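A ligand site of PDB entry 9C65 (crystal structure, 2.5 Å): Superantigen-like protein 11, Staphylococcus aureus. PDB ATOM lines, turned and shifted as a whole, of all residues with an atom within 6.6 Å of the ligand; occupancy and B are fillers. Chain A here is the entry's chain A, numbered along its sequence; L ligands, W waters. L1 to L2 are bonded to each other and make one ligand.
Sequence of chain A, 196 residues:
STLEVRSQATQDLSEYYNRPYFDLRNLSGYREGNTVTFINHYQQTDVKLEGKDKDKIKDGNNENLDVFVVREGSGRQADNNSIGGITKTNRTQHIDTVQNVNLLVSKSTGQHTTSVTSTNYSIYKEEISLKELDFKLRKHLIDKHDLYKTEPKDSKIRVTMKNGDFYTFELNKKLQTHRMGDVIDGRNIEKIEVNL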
ATOM      1  N   LEU A 130       3.885  34.741 -29.946  1.00  0.00           N
ATOM      2  CA  LEU A 130       4.170  33.588 -30.777  1.00  0.00           C
ATOM      3  C   LEU A 130       2.897  33.090 -31.452  1.00  0.00           C
ATOM      4  O   LEU A 130       2.907  32.510 -32.540  1.00  0.00           O
ATOM      5  CB  LEU A 130       4.827  32.470 -29.973  1.00  0.00           C
ATOM      6  CG  LEU A 130       6.188  32.816 -29.333  1.00  0.00           C
ATOM      7  CD1 LEU A 130       6.767  31.539 -28.711  1.00  0.00           C
ATOM      8  CD2 LEU A 130       7.217  33.423 -30.230  1.00  0.00           C
ATOM      9  N   ARG A 158      11.538  29.050 -38.123  1.00  0.00           N
ATOM     10  CA  ARG A 158      12.415  29.496 -37.053  1.00  0.00           C
ATOM     11  C   ARG A 158      12.568  31.011 -37.110  1.00  0.00           C
ATOM     12  O   ARG A 158      12.925  31.587 -38.144  1.00  0.00           O
ATOM     13  CB  ARG A 158      13.751  28.758 -37.023  1.00  0.00           C
ATOM     14  CG  ARG A 158      14.622  29.554 -36.058  1.00  0.00           C
ATOM     15  CD  ARG A 158      15.921  28.919 -35.718  1.00  0.00           C
ATOM     16  NE  ARG A 158      15.742  27.580 -35.155  1.00  0.00           N
ATOM     17  CZ  ARG A 158      16.810  26.816 -34.904  1.00  0.00           C
ATOM     18  NH1 ARG A 158      18.023  27.313 -35.064  1.00  0.00           N
ATOM     19  NH2 ARG A 158      16.655  25.586 -34.455  1.00  0.00           N
ATOM     20  N   ASP A 165      18.969  34.519 -29.657  1.00  0.00           N
ATOM     21  CA  ASP A 165      17.833  33.757 -29.168  1.00  0.00           C
ATOM     22  C   ASP A 165      16.919  33.382 -30.343  1.00  0.00           C
ATOM     23  O   ASP A 165      16.872  34.095 -31.353  1.00  0.00           O
ATOM     24  CB  ASP A 165      17.005  34.555 -28.185  1.00  0.00           C
ATOM     25  CG  ASP A 165      17.585  34.778 -26.788  1.00  0.00           C
ATOM     26  OD1 ASP A 165      18.619  34.159 -26.484  1.00  0.00           O
ATOM     27  OD2 ASP A 165      16.973  35.545 -25.986  1.00  0.00           O
ATOM     28  N   PHE A 166      16.217  32.265 -30.227  1.00  0.00           N
ATOM     29  CA  PHE A 166      15.358  31.834 -31.319  1.00  0.00           C
ATOM     30  C   PHE A 166      14.111  31.081 -30.838  1.00  0.00           C
ATOM     31  O   PHE A 166      14.025  30.549 -29.724  1.00  0.00           O
ATOM     32  CB  PHE A 166      16.236  31.081 -32.323  1.00  0.00           C
ATOM     33  CG  PHE A 166      16.684  29.692 -31.892  1.00  0.00           C
ATOM     34  CD1 PHE A 166      15.812  28.615 -31.956  1.00  0.00           C
ATOM     35  CD2 PHE A 166      18.009  29.458 -31.483  1.00  0.00           C
ATOM     36  CE1 PHE A 166      16.232  27.332 -31.581  1.00  0.00           C
ATOM     37  CE2 PHE A 166      18.398  28.189 -31.082  1.00  0.00           C
ATOM     38  CZ  PHE A 166      17.512  27.128 -31.125  1.00  0.00           C
ATOM     39  N   TYR A 167      13.111  31.046 -31.705  1.00  0.00           N
ATOM     40  CA  TYR A 167      11.869  30.352 -31.462  1.00  0.00           C
ATOM     41  C   TYR A 167      11.533  29.471 -32.663  1.00  0.00           C
ATOM     42  O   TYR A 167      11.445  29.929 -33.781  1.00  0.00           O
ATOM     43  CB  TYR A 167      10.819  31.438 -31.222  1.00  0.00           C
ATOM     44  CG  TYR A 167      11.219  32.397 -30.128  1.00  0.00           C
ATOM     45  CD1 TYR A 167      10.920  32.114 -28.820  1.00  0.00           C
ATOM     46  CD2 TYR A 167      11.955  33.551 -30.387  1.00  0.00           C
ATOM     47  CE1 TYR A 167      11.306  32.963 -27.800  1.00  0.00           C
ATOM     48  CE2 TYR A 167      12.383  34.385 -29.366  1.00  0.00           C
ATOM     49  CZ  TYR A 167      12.072  34.062 -28.076  1.00  0.00           C
ATOM     50  OH  TYR A 167      12.417  34.823 -27.033  1.00  0.00           O
ATOM     51  N   THR A 168      11.236  28.214 -32.392  1.00  0.00           N
ATOM     52  CA  THR A 168      10.927  27.232 -33.411  1.00  0.00           C
ATOM     53  C   THR A 168       9.445  26.891 -33.379  1.00  0.00           C
ATOM     54  O   THR A 168       8.864  26.652 -32.297  1.00  0.00           O
ATOM     55  CB  THR A 168      11.705  25.954 -33.159  1.00  0.00           C
ATOM     56  OG1 THR A 168      13.041  26.424 -33.109  1.00  0.00           O
ATOM     57  CG2 THR A 168      11.507  24.971 -34.291  1.00  0.00           C
ATOM     58  N   PHE A 169       8.896  26.785 -34.581  1.00  0.00           N
ATOM     59  CA  PHE A 169       7.549  26.297 -34.810  1.00  0.00           C
ATOM     60  C   PHE A 169       7.623  25.085 -35.723  1.00  0.00           C
ATOM     61  O   PHE A 169       8.087  25.174 -36.878  1.00  0.00           O
ATOM     62  CB  PHE A 169       6.644  27.334 -35.482  1.00  0.00           C
ATOM     63  CG  PHE A 169       6.586  28.671 -34.781  1.00  0.00           C
ATOM     64  CD1 PHE A 169       6.566  28.760 -33.401  1.00  0.00           C
ATOM     65  CD2 PHE A 169       6.474  29.822 -35.511  1.00  0.00           C
ATOM     66  CE1 PHE A 169       6.548  29.993 -32.795  1.00  0.00           C
ATOM     67  CE2 PHE A 169       6.399  31.072 -34.912  1.00  0.00           C
ATOM     68  CZ  PHE A 169       6.440  31.161 -33.552  1.00  0.00           C
ATOM     69  N   GLU A 170       7.218  23.946 -35.167  1.00  0.00           N
ATOM     70  CA  GLU A 170       7.164  22.722 -35.923  1.00  0.00           C
ATOM     71  C   GLU A 170       5.850  22.653 -36.670  1.00  0.00           C
ATOM     72  O   GLU A 170       4.796  22.602 -36.035  1.00  0.00           O
ATOM     73  CB  GLU A 170       7.257  21.509 -34.996  1.00  0.00           C
ATOM     74  CG  GLU A 170       8.641  21.312 -34.371  1.00  0.00           C
ATOM     75  CD  GLU A 170       8.680  20.033 -33.520  1.00  0.00           C
ATOM     76  OE1 GLU A 170       7.929  19.884 -32.467  1.00  0.00           O
ATOM     77  OE2 GLU A 170       9.503  19.164 -33.964  1.00  0.00           O
ATOM     78  N   LYS A 173       2.891  19.998 -36.168  1.00  0.00           N
ATOM     79  CA  LYS A 173       1.851  20.072 -35.128  1.00  0.00           C
ATOM     80  C   LYS A 173       1.429  21.516 -34.925  1.00  0.00           C
ATOM     81  O   LYS A 173       2.204  22.438 -35.152  1.00  0.00           O
ATOM     82  CB  LYS A 173       2.217  19.433 -33.775  1.00  0.00           C
ATOM     83  CG  LYS A 173       3.653  19.758 -33.279  1.00  0.00           C
ATOM     84  CD  LYS A 173       4.233  19.103 -32.013  1.00  0.00           C
ATOM     85  CE  LYS A 173       5.168  17.930 -32.214  1.00  0.00           C
ATOM     86  NZ  LYS A 173       6.099  18.047 -33.373  1.00  0.00           N
ATOM     87  N   LYS A 174       0.211  21.690 -34.376  1.00  0.00           N
ATOM     88  CA  LYS A 174      -0.193  23.002 -33.892  1.00  0.00           C
ATOM     89  C   LYS A 174       0.863  23.509 -32.920  1.00  0.00           C
ATOM     90  O   LYS A 174       1.575  22.697 -32.335  1.00  0.00           O
ATOM     91  CB  LYS A 174      -1.548  23.086 -33.224  1.00  0.00           C
ATOM     92  CG  LYS A 174      -2.701  22.752 -34.136  1.00  0.00           C
ATOM     93  CD  LYS A 174      -4.041  22.651 -33.420  1.00  0.00           C
ATOM     94  CE  LYS A 174      -4.142  23.736 -32.411  1.00  0.00           C
ATOM     95  NZ  LYS A 174      -5.543  23.951 -32.070  1.00  0.00           N
ATOM     96  N   LEU A 175       1.030  24.840 -32.861  1.00  0.00           N
ATOM     97  CA  LEU A 175       1.778  25.477 -31.816  1.00  0.00           C
ATOM     98  C   LEU A 175       1.254  25.009 -30.445  1.00  0.00           C
ATOM     99  O   LEU A 175       0.049  24.978 -30.214  1.00  0.00           O
ATOM    100  CB  LEU A 175       1.608  26.985 -31.906  1.00  0.00           C
ATOM    101  CG  LEU A 175       2.474  27.739 -30.900  1.00  0.00           C
ATOM    102  CD1 LEU A 175       3.919  27.345 -31.021  1.00  0.00           C
ATOM    103  CD2 LEU A 175       2.340  29.167 -31.045  1.00  0.00           C
ATOM    104  N   GLN A 176       2.167  24.703 -29.506  1.00  0.00           N
ATOM    105  CA  GLN A 176       1.772  24.226 -28.197  1.00  0.00           C
ATOM    106  C   GLN A 176       1.057  25.339 -27.486  1.00  0.00           C
ATOM    107  O   GLN A 176       1.547  26.462 -27.462  1.00  0.00           O
ATOM    108  CB  GLN A 176       2.990  23.796 -27.398  1.00  0.00           C
ATOM    109  CG  GLN A 176       3.723  22.609 -28.036  1.00  0.00           C
ATOM    110  CD  GLN A 176       4.820  22.992 -28.976  1.00  0.00           C
ATOM    111  OE1 GLN A 176       4.807  24.064 -29.589  1.00  0.00           O
ATOM    112  NE2 GLN A 176       5.835  22.152 -29.030  1.00  0.00           N
ATOM    113  N   HIS A 178       0.728  26.159 -24.439  1.00  0.00           N
ATOM    114  CA  HIS A 178       1.426  26.912 -23.389  1.00  0.00           C
ATOM    115  C   HIS A 178       2.355  28.009 -23.959  1.00  0.00           C
ATOM    116  O   HIS A 178       2.732  28.931 -23.201  1.00  0.00           O
ATOM    117  CB  HIS A 178       2.170  26.029 -22.386  1.00  0.00           C
ATOM    118  CG  HIS A 178       3.319  25.376 -22.990  1.00  0.00           C
ATOM    119  ND1 HIS A 178       3.100  24.270 -23.775  1.00  0.00           N
ATOM    120  CD2 HIS A 178       4.635  25.662 -23.016  1.00  0.00           C
ATOM    121  CE1 HIS A 178       4.272  23.857 -24.271  1.00  0.00           C
ATOM    122  NE2 HIS A 178       5.221  24.723 -23.861  1.00  0.00           N
ATOM    123  N   ARG A 179       2.674  27.920 -25.286  1.00  0.00           N
ATOM    124  CA  ARG A 179       3.494  28.913 -25.978  1.00  0.00           C
ATOM    125  C   ARG A 179       2.702  30.065 -26.635  1.00  0.00           C
ATOM    126  O   ARG A 179       3.295  31.145 -26.898  1.00  0.00           O
ATOM    127  CB  ARG A 179       4.336  28.193 -27.020  1.00  0.00           C
ATOM    128  CG  ARG A 179       5.243  27.141 -26.397  1.00  0.00           C
ATOM    129  CD  ARG A 179       6.034  26.417 -27.382  1.00  0.00           C
ATOM    130  NE  ARG A 179       7.040  27.242 -28.052  1.00  0.00           N
ATOM    131  CZ  ARG A 179       7.347  27.051 -29.336  1.00  0.00           C
ATOM    132  NH1 ARG A 179       6.830  26.009 -29.998  1.00  0.00           N
ATOM    133  NH2 ARG A 179       8.171  27.863 -29.971  1.00  0.00           N
ATOM    134  N   MET A 180       1.379  29.911 -26.794  1.00  0.00           N
ATOM    135  CA  MET A 180       0.565  30.894 -27.480  1.00  0.00           C
ATOM    136  C   MET A 180       0.585  32.259 -26.795  1.00  0.00           C
ATOM    137  O   MET A 180       0.348  33.332 -27.420  1.00  0.00           O
ATOM    138  CB  MET A 180      -0.861  30.414 -27.739  1.00  0.00           C
ATOM    139  CG  MET A 180      -0.853  29.210 -28.677  1.00  0.00           C
ATOM    140  SD  MET A 180      -2.553  28.625 -28.821  1.00  0.00           S
ATOM    141  CE  MET A 180      -2.454  27.480 -30.209  1.00  0.00           C
ATOM    142  N   ASP A 182       3.278  33.419 -25.020  1.00  0.00           N
ATOM    143  CA  ASP A 182       4.642  33.904 -24.919  1.00  0.00           C
ATOM    144  C   ASP A 182       4.815  35.028 -25.912  1.00  0.00           C
ATOM    145  O   ASP A 182       4.235  34.982 -26.995  1.00  0.00           O
ATOM    146  CB  ASP A 182       5.651  32.805 -25.214  1.00  0.00           C
ATOM    147  CG  ASP A 182       5.852  31.737 -24.108  1.00  0.00           C
ATOM    148  OD1 ASP A 182       5.447  31.971 -22.895  1.00  0.00           O
ATOM    149  OD2 ASP A 182       6.330  30.642 -24.505  1.00  0.00           O
HETATM  150  C1  LIG L   1      12.522  26.733 -29.332  1.00  0.00           C
HETATM  151  C2  LIG L   1      12.923  26.370 -27.889  1.00  0.00           C
HETATM  152  C3  LIG L   1      14.422  26.522 -27.715  1.00  0.00           C
HETATM  153  C4  LIG L   1      14.806  27.973 -27.799  1.00  0.00           C
HETATM  154  C5  LIG L   1      13.919  28.744 -26.827  1.00  0.00           C
HETATM  155  C6  LIG L   1      12.450  28.528 -27.200  1.00  0.00           C
HETATM  156  C7  LIG L   1      11.465  29.351 -26.397  1.00  0.00           C
HETATM  157  C8  LIG L   1      10.038  28.836 -26.544  1.00  0.00           C
HETATM  158  C9  LIG L   1       8.955  29.684 -25.897  1.00  0.00           C
HETATM  159  C10 LIG L   1      14.441  30.999 -25.871  1.00  0.00           C
HETATM  160  C11 LIG L   1      14.047  30.580 -24.488  1.00  0.00           C
HETATM  161  N1  LIG L   1      14.229  30.171 -26.882  1.00  0.00           N
HETATM  162  O1  LIG L   1      11.399  27.110 -29.648  1.00  0.00           O
HETATM  163  O2  LIG L   1      13.352  26.602 -30.149  1.00  0.00           O
HETATM  164  O3  LIG L   1      16.216  28.156 -27.561  1.00  0.00           O
HETATM  165  O4  LIG L   1      12.147  27.131 -26.953  1.00  0.00           O
HETATM  166  O5  LIG L   1      11.872  29.230 -25.044  1.00  0.00           O
HETATM  167  O6  LIG L   1       9.761  28.751 -27.920  1.00  0.00           O
HETATM  168  O7  LIG L   1       7.629  29.199 -26.184  1.00  0.00           O
HETATM  169  O8  LIG L   1      14.896  32.131 -26.095  1.00  0.00           O
HETATM  170  C1  LG2 L   2      10.985  24.554 -28.034  1.00  0.00           C
HETATM  171  C2  LG2 L   2      10.934  23.750 -29.286  1.00  0.00           C
HETATM  172  C3  LG2 L   2       9.469  22.533 -30.771  1.00  0.00           C
HETATM  173  C4  LG2 L   2       8.923  21.772 -25.340  1.00  0.00           C
HETATM  174  C5  LG2 L   2       7.852  21.191 -24.811  1.00  0.00           C
HETATM  175  C6  LG2 L   2       7.820  19.963 -23.839  1.00  0.00           C
HETATM  176  C7  LG2 L   2       9.088  23.675 -27.002  1.00  0.00           C
HETATM  177  N1  LG2 L   2       8.504  22.797 -26.076  1.00  0.00           N
HETATM  178  N2  LG2 L   2       6.763  21.807 -25.252  1.00  0.00           N
HETATM  179  O1  LG2 L   2      10.582  24.896 -25.718  1.00  0.00           O
HETATM  180  C8  LG2 L   2      10.461  23.906 -26.775  1.00  0.00           C
HETATM  181  O2  LG2 L   2      12.368  25.036 -27.759  1.00  0.00           O
HETATM  182  O3  LG2 L   2      11.879  22.803 -29.143  1.00  0.00           O
HETATM  183  C9  LG2 L   2       9.596  23.311 -29.485  1.00  0.00           C
HETATM  184  O4  LG2 L   2       8.004  22.164 -31.056  1.00  0.00           O
HETATM  185  O5  LG2 L   2       9.039  22.661 -28.241  1.00  0.00           O
HETATM  186  N3  LG2 L   2       7.195  22.786 -26.028  1.00  0.00           N
HETATM  187  O6  LG2 L   2       9.053  19.808 -23.161  1.00  0.00           O
HETATM  188  O   HOH W   1      17.375  30.433 -28.184  1.00  0.00           O
HETATM  189  O   HOH W   2       7.434  28.702 -22.878  1.00  0.00           O
HETATM  190  O   HOH W   3       6.535  24.099 -32.439  1.00  0.00           O
HETATM  191  O   HOH W   4      18.054  25.789 -28.064  1.00  0.00           O
HETATM  192  O   HOH W   5      16.240  28.156 -23.582  1.00  0.00           O
HETATM  193  O   HOH W   6       4.897  20.272 -25.369  1.00  0.00           O
HETATM  194  O   HOH W   7      12.705  26.091 -24.355  1.00  0.00           O
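Residues that only touch the ligand: Leu 130 (3.6 Å), Asp 165 (3.8 Å), Tyr 167 (3.7 Å) and His 178 (3.4 Å).
Hydrophobic or aromatic side chains that line the ligand: Leu 130, Phe 166, Tyr 167 and His 178.
Ten residues have an atom within 4 Å of the ligand: Leu 130, Asp 165, Phe 166, Tyr 167, Thr 168, Glu 170, Gln 176, His 178, Arg 179 and Asp 182.
Water W1 lies within hydrogen-bond range of O3 of LIG L1 (2.6 Å) and N of Phe 166 (3.0 Å).
Water W3 lies within hydrogen-bond range of O4 of LG2 L2, N of Glu 170, NH1 of Arg 179, OE1 of Gln 176 and O of Thr 168.
Water W2 lies within hydrogen-bond range of the side-chain carboxylate (OD2) of Asp 182 (2.8 Å) and an oxygen (O7) of LIG L1 (3.3 Å).
An oxygen (O7) of LIG L1 is in hydrogen-bond range of the side-chain carboxylate of Asp 182 (2.6 Å).
An oxygen (O4) of LG2 L2 sits at hydrogen-bond distance from the side-chain carboxylate of Glu 170.
The guanidinium group (NH2) of Arg 179 lies within salt-bridge range of an oxygen (O1) of LIG L1 (3.3 Å).
O of Phe 166 lies within hydrogen-bond range of N1 of LIG L1 (2.9 Å).
N of Thr 168 is in hydrogen-bond range of O1 of LIG L1 (3.0 Å).
The side-chain hydroxyl (OG1) of Thr 168 is in hydrogen-bond range of an oxygen (O2) of LIG L1 (3.0 Å).
O4 of LG2 L2 sits at hydrogen-bond distance from NE2 of Gln 176 (3.0 Å).
The backbone carbonyl oxygen (O) of Asp 182 lies within hydrogen-bond range of the backbone NH (N) of Leu 130 (3.0 Å).
The side-chain amino group of Lys 173 lies within salt-bridge range of the side-chain carboxylate of Glu 170, 2.7 Å away.
O of Thr 168 sits at hydrogen-bond distance from NH2 of Arg 179.
The guanidinium group (NH1) of Arg 179 lies within hydrogen-bond range of the side-chain amide oxygen (OE1) of Gln 176 (2.8 Å).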
